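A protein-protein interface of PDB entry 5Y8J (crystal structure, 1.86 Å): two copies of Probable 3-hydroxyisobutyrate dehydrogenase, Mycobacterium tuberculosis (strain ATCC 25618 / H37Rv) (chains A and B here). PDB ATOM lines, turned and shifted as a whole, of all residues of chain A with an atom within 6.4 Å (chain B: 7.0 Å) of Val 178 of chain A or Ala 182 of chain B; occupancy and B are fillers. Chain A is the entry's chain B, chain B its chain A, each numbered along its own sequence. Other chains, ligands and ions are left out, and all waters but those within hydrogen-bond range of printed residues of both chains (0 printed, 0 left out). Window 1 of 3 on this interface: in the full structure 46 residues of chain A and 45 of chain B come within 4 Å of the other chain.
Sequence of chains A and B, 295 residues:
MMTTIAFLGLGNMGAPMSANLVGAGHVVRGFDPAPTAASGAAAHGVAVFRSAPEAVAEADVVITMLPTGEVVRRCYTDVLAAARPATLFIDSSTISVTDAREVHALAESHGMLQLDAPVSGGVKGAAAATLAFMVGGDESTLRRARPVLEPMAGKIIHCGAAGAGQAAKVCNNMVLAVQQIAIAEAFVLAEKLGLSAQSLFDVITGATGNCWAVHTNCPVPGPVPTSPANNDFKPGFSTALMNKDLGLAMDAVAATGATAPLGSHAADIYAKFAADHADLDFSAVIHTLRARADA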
ATOM      1  N   CYS A 171      -4.480  26.501 -32.952  1.00  0.00           N
ATOM      2  CA  CYS A 171      -2.990  26.426 -33.071  1.00  0.00           C
ATOM      3  C   CYS A 171      -2.352  27.826 -33.044  1.00  0.00           C
ATOM      4  O   CYS A 171      -1.406  28.073 -32.277  1.00  0.00           O
ATOM      5  CB  CYS A 171      -2.602  25.694 -34.347  1.00  0.00           C
ATOM      6  SG  CYS A 171      -2.886  23.906 -34.277  1.00  0.00           S
ATOM      7  N   ASN A 173      -3.661  30.509 -31.741  1.00  0.00           N
ATOM      8  CA  ASN A 173      -3.852  31.246 -30.475  1.00  0.00           C
ATOM      9  C   ASN A 173      -3.002  30.660 -29.304  1.00  0.00           C
ATOM     10  O   ASN A 173      -2.728  31.329 -28.283  1.00  0.00           O
ATOM     11  CB  ASN A 173      -5.360  31.335 -30.131  1.00  0.00           C
ATOM     12  CG  ASN A 173      -6.088  32.450 -30.956  1.00  0.00           C
ATOM     13  OD1 ASN A 173      -5.535  33.040 -31.919  1.00  0.00           O
ATOM     14  ND2 ASN A 173      -7.299  32.752 -30.573  1.00  0.00           N
ATOM     15  N   MET A 174      -2.723  29.386 -29.409  1.00  0.00           N
ATOM     16  CA  MET A 174      -1.844  28.707 -28.428  1.00  0.00           C
ATOM     17  C   MET A 174      -0.447  29.379 -28.594  1.00  0.00           C
ATOM     18  O   MET A 174       0.201  29.769 -27.619  1.00  0.00           O
ATOM     19  CB  MET A 174      -1.719  27.195 -28.720  1.00  0.00           C
ATOM     20  CG  MET A 174      -0.910  26.424 -27.642  1.00  0.00           C
ATOM     21  SD  MET A 174      -0.879  24.629 -27.884  1.00  0.00           S
ATOM     22  CE  MET A 174       0.025  24.453 -29.390  1.00  0.00           C
ATOM     23  N   VAL A 175       0.006  29.451 -29.806  1.00  0.00           N
ATOM     24  CA  VAL A 175       1.248  30.178 -30.096  1.00  0.00           C
ATOM     25  C   VAL A 175       1.235  31.638 -29.542  1.00  0.00           C
ATOM     26  O   VAL A 175       2.179  32.058 -28.866  1.00  0.00           O
ATOM     27  CB  VAL A 175       1.586  30.188 -31.582  1.00  0.00           C
ATOM     28  CG1 VAL A 175       2.742  31.136 -31.862  1.00  0.00           C
ATOM     29  CG2 VAL A 175       1.878  28.815 -32.080  1.00  0.00           C
ATOM     30  N   LEU A 176       0.160  32.362 -29.825  1.00  0.00           N
ATOM     31  CA  LEU A 176      -0.019  33.692 -29.267  1.00  0.00           C
ATOM     32  C   LEU A 176       0.092  33.807 -27.769  1.00  0.00           C
ATOM     33  O   LEU A 176       0.834  34.636 -27.284  1.00  0.00           O
ATOM     34  CB  LEU A 176      -1.326  34.279 -29.778  1.00  0.00           C
ATOM     35  CG  LEU A 176      -1.628  35.683 -29.220  1.00  0.00           C
ATOM     36  CD1 LEU A 176      -0.639  36.682 -29.752  1.00  0.00           C
ATOM     37  CD2 LEU A 176      -3.043  35.990 -29.668  1.00  0.00           C
ATOM     38  N   ALA A 177      -0.582  32.905 -27.020  1.00  0.00           N
ATOM     39  CA  ALA A 177      -0.490  32.861 -25.618  1.00  0.00           C
ATOM     40  C   ALA A 177       0.931  32.651 -25.124  1.00  0.00           C
ATOM     41  O   ALA A 177       1.381  33.331 -24.158  1.00  0.00           O
ATOM     42  CB  ALA A 177      -1.372  31.752 -25.097  1.00  0.00           C
ATOM     43  N   VAL A 178       1.621  31.703 -25.701  1.00  0.00           N
ATOM     44  CA  VAL A 178       3.039  31.461 -25.327  1.00  0.00           C
ATOM     45  C   VAL A 178       3.898  32.741 -25.603  1.00  0.00           C
ATOM     46  O   VAL A 178       4.679  33.164 -24.750  1.00  0.00           O
ATOM     47  CB  VAL A 178       3.567  30.293 -26.140  1.00  0.00           C
ATOM     48  CG1 VAL A 178       5.086  30.099 -25.988  1.00  0.00           C
ATOM     49  CG2 VAL A 178       2.868  28.982 -25.749  1.00  0.00           C
ATOM     50  N   GLN A 179       3.680  33.371 -26.754  1.00  0.00           N
ATOM     51  CA  GLN A 179       4.457  34.566 -27.113  1.00  0.00           C
ATOM     52  C   GLN A 179       4.143  35.693 -26.183  1.00  0.00           C
ATOM     53  O   GLN A 179       5.013  36.436 -25.816  1.00  0.00           O
ATOM     54  CB  GLN A 179       4.131  35.009 -28.530  1.00  0.00           C
ATOM     55  CG  GLN A 179       4.676  34.085 -29.600  1.00  0.00           C
ATOM     56  CD  GLN A 179       4.027  34.300 -30.961  1.00  0.00           C
ATOM     57  OE1 GLN A 179       2.882  34.802 -31.066  1.00  0.00           O
ATOM     58  NE2 GLN A 179       4.746  33.960 -32.025  1.00  0.00           N
ATOM     59  N   GLN A 180       2.875  35.846 -25.812  1.00  0.00           N
ATOM     60  CA  GLN A 180       2.496  36.938 -24.901  1.00  0.00           C
ATOM     61  C   GLN A 180       3.129  36.801 -23.521  1.00  0.00           C
ATOM     62  O   GLN A 180       3.586  37.809 -22.916  1.00  0.00           O
ATOM     63  CB  GLN A 180       0.976  37.109 -24.772  1.00  0.00           C
ATOM     64  CG  GLN A 180       0.564  38.427 -24.087  1.00  0.00           C
ATOM     65  CD  GLN A 180       0.841  39.664 -24.964  1.00  0.00           C
ATOM     66  OE1 GLN A 180       0.254  39.804 -26.054  1.00  0.00           O
ATOM     67  NE2 GLN A 180       1.862  40.420 -24.620  1.00  0.00           N
ATOM     68  N   ILE A 181       3.208  35.593 -23.028  1.00  0.00           N
ATOM     69  CA  ILE A 181       3.923  35.362 -21.743  1.00  0.00           C
ATOM     70  C   ILE A 181       5.445  35.624 -21.932  1.00  0.00           C
ATOM     71  O   ILE A 181       6.082  36.265 -21.115  1.00  0.00           O
ATOM     72  CB  ILE A 181       3.674  33.938 -21.234  1.00  0.00           C
ATOM     73  CG1 ILE A 181       2.185  33.808 -20.815  1.00  0.00           C
ATOM     74  CG2 ILE A 181       4.578  33.673 -20.024  1.00  0.00           C
ATOM     75  CD1 ILE A 181       1.674  32.387 -20.718  1.00  0.00           C
ATOM     76  N   ALA A 182       6.002  35.064 -23.008  1.00  0.00           N
ATOM     77  CA  ALA A 182       7.438  35.184 -23.213  1.00  0.00           C
ATOM     78  C   ALA A 182       7.918  36.644 -23.376  1.00  0.00           C
ATOM     79  O   ALA A 182       8.974  36.948 -22.901  1.00  0.00           O
ATOM     80  CB  ALA A 182       7.881  34.347 -24.411  1.00  0.00           C
ATOM     81  N   ILE A 183       7.158  37.465 -24.093  1.00  0.00           N
ATOM     82  CA  ILE A 183       7.401  38.869 -24.218  1.00  0.00           C
ATOM     83  C   ILE A 183       7.322  39.514 -22.836  1.00  0.00           C
ATOM     84  O   ILE A 183       8.173  40.304 -22.473  1.00  0.00           O
ATOM     85  CB  ILE A 183       6.459  39.512 -25.215  1.00  0.00           C
ATOM     86  CG1 ILE A 183       6.804  39.119 -26.676  1.00  0.00           C
ATOM     87  CG2 ILE A 183       6.409  41.026 -25.103  1.00  0.00           C
ATOM     88  CD1 ILE A 183       8.203  39.524 -27.182  1.00  0.00           C
ATOM     89  N   LEU A 246      -7.241  28.508 -24.809  1.00  0.00           N
ATOM     90  CA  LEU A 246      -6.229  27.589 -24.332  1.00  0.00           C
ATOM     91  C   LEU A 246      -6.863  26.262 -23.824  1.00  0.00           C
ATOM     92  O   LEU A 246      -6.294  25.204 -24.015  1.00  0.00           O
ATOM     93  CB  LEU A 246      -5.342  28.271 -23.292  1.00  0.00           C
ATOM     94  CG  LEU A 246      -4.399  29.286 -23.915  1.00  0.00           C
ATOM     95  CD1 LEU A 246      -3.715  30.092 -22.842  1.00  0.00           C
ATOM     96  CD2 LEU A 246      -3.366  28.636 -24.807  1.00  0.00           C
ATOM     97  N   LEU A 262       5.201  23.938 -23.863  1.00  0.00           N
ATOM     98  CA  LEU A 262       5.046  25.338 -23.598  1.00  0.00           C
ATOM     99  C   LEU A 262       3.596  25.736 -23.723  1.00  0.00           C
ATOM    100  O   LEU A 262       3.126  26.556 -22.943  1.00  0.00           O
ATOM    101  CB  LEU A 262       5.940  26.201 -24.489  1.00  0.00           C
ATOM    102  CG  LEU A 262       7.444  25.864 -24.400  1.00  0.00           C
ATOM    103  CD1 LEU A 262       8.310  26.941 -25.074  1.00  0.00           C
ATOM    104  CD2 LEU A 262       7.905  25.750 -22.964  1.00  0.00           C
ATOM    105  N   GLY A 263       2.886  25.199 -24.714  1.00  0.00           N
ATOM    106  CA  GLY A 263       1.466  25.524 -24.851  1.00  0.00           C
ATOM    107  C   GLY A 263       0.697  25.103 -23.611  1.00  0.00           C
ATOM    108  O   GLY A 263      -0.151  25.863 -23.105  1.00  0.00           O
ATOM    109  N   SER A 264       1.004  23.928 -23.104  1.00  0.00           N
ATOM    110  CA  SER A 264       0.332  23.436 -21.858  1.00  0.00           C
ATOM    111  C   SER A 264       0.740  24.246 -20.607  1.00  0.00           C
ATOM    112  O   SER A 264      -0.101  24.550 -19.726  1.00  0.00           O
ATOM    113  CB  SER A 264       0.563  21.978 -21.642  1.00  0.00           C
ATOM    114  OG  SER A 264       0.281  21.250 -22.809  1.00  0.00           O
ATOM    115  N   ALA A 266       1.630  27.417 -20.837  1.00  0.00           N
ATOM    116  CA  ALA A 266       0.917  28.644 -21.003  1.00  0.00           C
ATOM    117  C   ALA A 266      -0.566  28.533 -20.579  1.00  0.00           C
ATOM    118  O   ALA A 266      -1.118  29.466 -20.004  1.00  0.00           O
ATOM    119  CB  ALA A 266       1.039  29.145 -22.423  1.00  0.00           C
ATOM    120  N   TYR A 270      -2.404  30.810 -17.690  1.00  0.00           N
ATOM    121  CA  TYR A 270      -3.586  31.624 -18.034  1.00  0.00           C
ATOM    122  C   TYR A 270      -4.824  31.164 -17.231  1.00  0.00           C
ATOM    123  O   TYR A 270      -5.633  32.007 -16.811  1.00  0.00           O
ATOM    124  CB  TYR A 270      -3.797  31.657 -19.538  1.00  0.00           C
ATOM    125  CG  TYR A 270      -3.122  32.861 -20.182  1.00  0.00           C
ATOM    126  CD1 TYR A 270      -3.497  34.167 -19.776  1.00  0.00           C
ATOM    127  CD2 TYR A 270      -2.070  32.697 -21.084  1.00  0.00           C
ATOM    128  CE1 TYR A 270      -2.889  35.273 -20.320  1.00  0.00           C
ATOM    129  CE2 TYR A 270      -1.443  33.812 -21.642  1.00  0.00           C
ATOM    130  CZ  TYR A 270      -1.843  35.066 -21.241  1.00  0.00           C
ATOM    131  OH  TYR A 270      -1.173  36.120 -21.805  1.00  0.00           O
ATOM    132  N   LEU B 176      13.095  34.148 -28.631  1.00  0.00           N
ATOM    133  CA  LEU B 176      13.267  33.367 -29.886  1.00  0.00           C
ATOM    134  C   LEU B 176      13.174  31.857 -29.621  1.00  0.00           C
ATOM    135  O   LEU B 176      12.537  31.133 -30.375  1.00  0.00           O
ATOM    136  CB  LEU B 176      14.604  33.679 -30.550  1.00  0.00           C
ATOM    137  CG  LEU B 176      14.905  32.891 -31.805  1.00  0.00           C
ATOM    138  CD1 LEU B 176      13.855  33.061 -32.881  1.00  0.00           C
ATOM    139  CD2 LEU B 176      16.225  33.345 -32.379  1.00  0.00           C
ATOM    140  N   ALA B 177      13.845  31.379 -28.555  1.00  0.00           N
ATOM    141  CA  ALA B 177      13.840  29.950 -28.240  1.00  0.00           C
ATOM    142  C   ALA B 177      12.414  29.506 -27.908  1.00  0.00           C
ATOM    143  O   ALA B 177      11.968  28.475 -28.335  1.00  0.00           O
ATOM    144  CB  ALA B 177      14.762  29.681 -27.051  1.00  0.00           C
ATOM    145  N   VAL B 178      11.734  30.285 -27.107  1.00  0.00           N
ATOM    146  CA  VAL B 178      10.366  29.981 -26.751  1.00  0.00           C
ATOM    147  C   VAL B 178       9.518  29.900 -28.025  1.00  0.00           C
ATOM    148  O   VAL B 178       8.797  28.982 -28.222  1.00  0.00           O
ATOM    149  CB  VAL B 178       9.830  31.043 -25.780  1.00  0.00           C
ATOM    150  CG1 VAL B 178       8.315  30.987 -25.641  1.00  0.00           C
ATOM    151  CG2 VAL B 178      10.547  30.919 -24.443  1.00  0.00           C
ATOM    152  N   GLN B 179       9.656  30.897 -28.875  1.00  0.00           N
ATOM    153  CA  GLN B 179       8.927  30.952 -30.128  1.00  0.00           C
ATOM    154  C   GLN B 179       9.257  29.765 -31.029  1.00  0.00           C
ATOM    155  O   GLN B 179       8.361  29.211 -31.646  1.00  0.00           O
ATOM    156  CB  GLN B 179       9.195  32.258 -30.901  1.00  0.00           C
ATOM    157  CG  GLN B 179       8.661  33.512 -30.196  1.00  0.00           C
ATOM    158  CD  GLN B 179       9.167  34.754 -30.853  1.00  0.00           C
ATOM    159  OE1 GLN B 179      10.235  34.741 -31.434  1.00  0.00           O
ATOM    160  NE2 GLN B 179       8.409  35.863 -30.751  1.00  0.00           N
ATOM    161  N   GLN B 180      10.533  29.333 -31.086  1.00  0.00           N
ATOM    162  CA  GLN B 180      10.857  28.206 -31.959  1.00  0.00           C
ATOM    163  C   GLN B 180      10.232  26.932 -31.448  1.00  0.00           C
ATOM    164  O   GLN B 180       9.769  26.129 -32.253  1.00  0.00           O
ATOM    165  CB  GLN B 180      12.372  28.073 -32.192  1.00  0.00           C
ATOM    166  CG  GLN B 180      12.752  27.152 -33.345  1.00  0.00           C
ATOM    167  CD  GLN B 180      12.466  27.756 -34.730  1.00  0.00           C
ATOM    168  OE1 GLN B 180      13.011  28.762 -35.104  1.00  0.00           O
ATOM    169  NE2 GLN B 180      11.524  27.194 -35.429  1.00  0.00           N
ATOM    170  N   ILE B 181      10.131  26.771 -30.127  1.00  0.00           N
ATOM    171  CA  ILE B 181       9.491  25.594 -29.644  1.00  0.00           C
ATOM    172  C   ILE B 181       7.964  25.668 -29.863  1.00  0.00           C
ATOM    173  O   ILE B 181       7.315  24.676 -30.170  1.00  0.00           O
ATOM    174  CB  ILE B 181       9.795  25.420 -28.139  1.00  0.00           C
ATOM    175  CG1 ILE B 181      11.301  25.082 -27.990  1.00  0.00           C
ATOM    176  CG2 ILE B 181       8.949  24.273 -27.519  1.00  0.00           C
ATOM    177  CD1 ILE B 181      11.856  25.332 -26.623  1.00  0.00           C
ATOM    178  N   ALA B 182       7.405  26.800 -29.513  1.00  0.00           N
ATOM    179  CA  ALA B 182       5.974  27.008 -29.658  1.00  0.00           C
ATOM    180  C   ALA B 182       5.498  26.710 -31.097  1.00  0.00           C
ATOM    181  O   ALA B 182       4.546  26.044 -31.291  1.00  0.00           O
ATOM    182  CB  ALA B 182       5.554  28.382 -29.200  1.00  0.00           C
ATOM    183  N   ILE B 183       6.219  27.207 -32.077  1.00  0.00           N
ATOM    184  CA  ILE B 183       5.903  26.957 -33.452  1.00  0.00           C
ATOM    185  C   ILE B 183       6.001  25.478 -33.766  1.00  0.00           C
ATOM    186  O   ILE B 183       5.170  24.925 -34.563  1.00  0.00           O
ATOM    187  CB  ILE B 183       6.827  27.781 -34.392  1.00  0.00           C
ATOM    188  CG1 ILE B 183       6.433  29.289 -34.341  1.00  0.00           C
ATOM    189  CG2 ILE B 183       6.854  27.277 -35.812  1.00  0.00           C
ATOM    190  CD1 ILE B 183       5.053  29.645 -34.819  1.00  0.00           C
ATOM    191  N   ALA B 184       7.040  24.816 -33.234  1.00  0.00           N
ATOM    192  CA  ALA B 184       7.127  23.399 -33.460  1.00  0.00           C
ATOM    193  C   ALA B 184       5.904  22.639 -32.894  1.00  0.00           C
ATOM    194  O   ALA B 184       5.323  21.766 -33.538  1.00  0.00           O
ATOM    195  CB  ALA B 184       8.424  22.834 -32.851  1.00  0.00           C
ATOM    196  N   GLU B 185       5.543  22.993 -31.673  1.00  0.00           N
ATOM    197  CA  GLU B 185       4.330  22.398 -31.058  1.00  0.00           C
ATOM    198  C   GLU B 185       3.094  22.578 -31.929  1.00  0.00           C
ATOM    199  O   GLU B 185       2.286  21.635 -32.082  1.00  0.00           O
ATOM    200  CB  GLU B 185       4.032  23.006 -29.701  1.00  0.00           C
ATOM    201  CG  GLU B 185       5.099  22.741 -28.666  1.00  0.00           C
ATOM    202  CD  GLU B 185       4.838  23.495 -27.324  1.00  0.00           C
ATOM    203  OE1 GLU B 185       3.794  24.172 -27.102  1.00  0.00           O
ATOM    204  OE2 GLU B 185       5.770  23.435 -26.483  1.00  0.00           O
ATOM    205  N   ALA B 186       2.949  23.776 -32.441  1.00  0.00           N
ATOM    206  CA  ALA B 186       1.818  24.107 -33.312  1.00  0.00           C
ATOM    207  C   ALA B 186       1.797  23.300 -34.611  1.00  0.00           C
ATOM    208  O   ALA B 186       0.736  22.803 -35.001  1.00  0.00           O
ATOM    209  CB  ALA B 186       1.794  25.586 -33.614  1.00  0.00           C
ATOM    210  N   PHE B 187       2.916  23.115 -35.283  1.00  0.00           N
ATOM    211  CA  PHE B 187       2.955  22.263 -36.473  1.00  0.00           C
ATOM    212  C   PHE B 187       2.648  20.795 -36.172  1.00  0.00           C
ATOM    213  O   PHE B 187       1.950  20.156 -36.953  1.00  0.00           O
ATOM    214  CB  PHE B 187       4.273  22.376 -37.277  1.00  0.00           C
ATOM    215  CG  PHE B 187       4.269  23.535 -38.179  1.00  0.00           C
ATOM    216  CD1 PHE B 187       3.638  23.463 -39.408  1.00  0.00           C
ATOM    217  CD2 PHE B 187       4.753  24.788 -37.739  1.00  0.00           C
ATOM    218  CE1 PHE B 187       3.552  24.571 -40.222  1.00  0.00           C
ATOM    219  CE2 PHE B 187       4.708  25.875 -38.576  1.00  0.00           C
ATOM    220  CZ  PHE B 187       4.076  25.773 -39.827  1.00  0.00           C
ATOM    221  N   ILE B 204      -0.990  31.113 -39.752  1.00  0.00           N
ATOM    222  CA  ILE B 204      -0.137  31.746 -38.746  1.00  0.00           C
ATOM    223  C   ILE B 204       0.618  32.952 -39.280  1.00  0.00           C
ATOM    224  O   ILE B 204       0.697  33.950 -38.656  1.00  0.00           O
ATOM    225  CB  ILE B 204       0.880  30.786 -38.134  1.00  0.00           C
ATOM    226  CG1 ILE B 204       0.181  29.646 -37.442  1.00  0.00           C
ATOM    227  CG2 ILE B 204       1.749  31.545 -37.177  1.00  0.00           C
ATOM    228  CD1 ILE B 204       1.008  28.930 -36.404  1.00  0.00           C
ATOM    229  N   LEU B 262       8.412  30.365 -18.906  1.00  0.00           N
ATOM    230  CA  LEU B 262       8.531  29.761 -20.205  1.00  0.00           C
ATOM    231  C   LEU B 262       9.984  29.798 -20.781  1.00  0.00           C
ATOM    232  O   LEU B 262      10.431  28.860 -21.381  1.00  0.00           O
ATOM    233  CB  LEU B 262       7.580  30.383 -21.214  1.00  0.00           C
ATOM    234  CG  LEU B 262       6.086  30.214 -20.923  1.00  0.00           C
ATOM    235  CD1 LEU B 262       5.252  30.632 -22.133  1.00  0.00           C
ATOM    236  CD2 LEU B 262       5.699  28.819 -20.456  1.00  0.00           C
ATOM    237  N   VAL B 285      14.297  21.030 -32.771  1.00  0.00           N
ATOM    238  CA  VAL B 285      13.534  20.734 -31.565  1.00  0.00           C
ATOM    239  C   VAL B 285      12.159  20.123 -31.799  1.00  0.00           C
ATOM    240  O   VAL B 285      11.578  19.501 -30.878  1.00  0.00           O
ATOM    241  CB  VAL B 285      13.469  22.013 -30.743  1.00  0.00           C
ATOM    242  CG1 VAL B 285      12.413  22.944 -31.274  1.00  0.00           C
ATOM    243  CG2 VAL B 285      13.335  21.687 -29.267  1.00  0.00           C
ATOM    244  N   LEU B 289      10.101  16.590 -29.011  1.00  0.00           N
ATOM    245  CA  LEU B 289       8.994  16.874 -28.131  1.00  0.00           C
ATOM    246  C   LEU B 289       8.423  15.633 -27.479  1.00  0.00           C
ATOM    247  O   LEU B 289       7.897  15.721 -26.439  1.00  0.00           O
ATOM    248  CB  LEU B 289       7.913  17.671 -28.840  1.00  0.00           C
ATOM    249  CG  LEU B 289       8.216  19.032 -29.456  1.00  0.00           C
ATOM    250  CD1 LEU B 289       7.059  19.534 -30.287  1.00  0.00           C
ATOM    251  CD2 LEU B 289       8.599  20.038 -28.417  1.00  0.00           C
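Of the 16 printed residues of chain B, 6 touch a printed residue of chain A.
Printed residues of chain B that touch a printed residue of chain A: Val 178, Ile 181, Ala 182, Glu 185, Ala 186 and Leu 262.
Of the 18 printed residues of chain A, 7 touch a printed residue of chain B.
Hydrophobic or aromatic side chains of chain A within 4 Å of the printed part of chain B: Val 175, Val 178, Ile 181, Ala 182 and Leu 262.
Among the printed residues, 12 pairs touch across the chains.
Val 178 of chain A touches just these residues of chain B: Val 178 (3.4 Å), Ala 182 (3.7 Å) and Leu 262 (3.7 Å).
Of chain A, only Val 175 (3.9 Å) and Val 178 (3.7 Å) come within 4 Å of Ala 182 of chain B.
Of the printed residues of chain A, Glu 185 of chain B touches Leu 262 and Gly 263.
Of the printed residues of chain A, Ala 186 of chain B touches Cys 171 and Val 175.
Of the printed residues of chain B, Leu 262 of chain A touches Val 178 (3.8 Å), Ile 181 (3.7 Å) and Glu 185 (2.7 Å).
Of the printed residues of chain B, Ala 182 of chain A touches Val 178 (3.6 Å).
Of the printed residues of chain B, Val 175 of chain A touches Ala 182 and Ala 186.
The nearest residue of chain A that does not touch Ala 182 of chain B is Leu 262 of chain A (4.5 Å).
The side-chain carboxylate (OE2) of Glu 185 of chain B lies within hydrogen-bond range of the backbone NH (N) of Leu 262 of chain A (2.7 Å).
The side-chain carboxylate of Glu 185 of chain B sits at hydrogen-bond distance from the backbone NH of Gly 263 of chain A, at 2.8 Å.
Val 178 of chain A touches its own counterpart, Val 178 of chain B.
Val 178 of chain A touches Ala 182 of chain B, and with the chains exchanged Ala 182 of chain A touches Val 178 of chain B.
Val 178 of chain A touches Leu 262 of chain B, and with the chains exchanged Leu 262 of chain A touches Val 178 of chain B.
Ile 181 of chain A touches Leu 262 of chain B, and with the chains exchanged Leu 262 of chain A touches Ile 181 of chain B.
O of Ala 186 of chain B touches SG of Cys 171 of chain A (3.9 Å).
Val 175 of chain A touches Ala 182 of chain B (CG2 to O, 3.9 Å).
Val 175 of chain A touches Ala 186 of chain B (CG2 to CB, 3.6 Å).
CG1 of Val 178 of chain A touches CG1 of Val 178 of chain B, 3.4 Å away.
CG1 of Val 178 of chain A touches CB of Ala 182 of chain B, 3.7 Å away.
Leu 262 of chain B touches Val 178 of chain A (CD1 to O, 3.7 Å).
CG2 of Ile 181 of chain A touches CD1 of Leu 262 of chain B (3.8 Å).
Ala 182 of chain A touches Val 178 of chain B.
Val 178 of chain B touches Leu 262 of chain A (O to CD1, 3.8 Å).
CD1 of Leu 262 of chain A touches CG2 of Ile 181 of chain B (3.7 Å).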
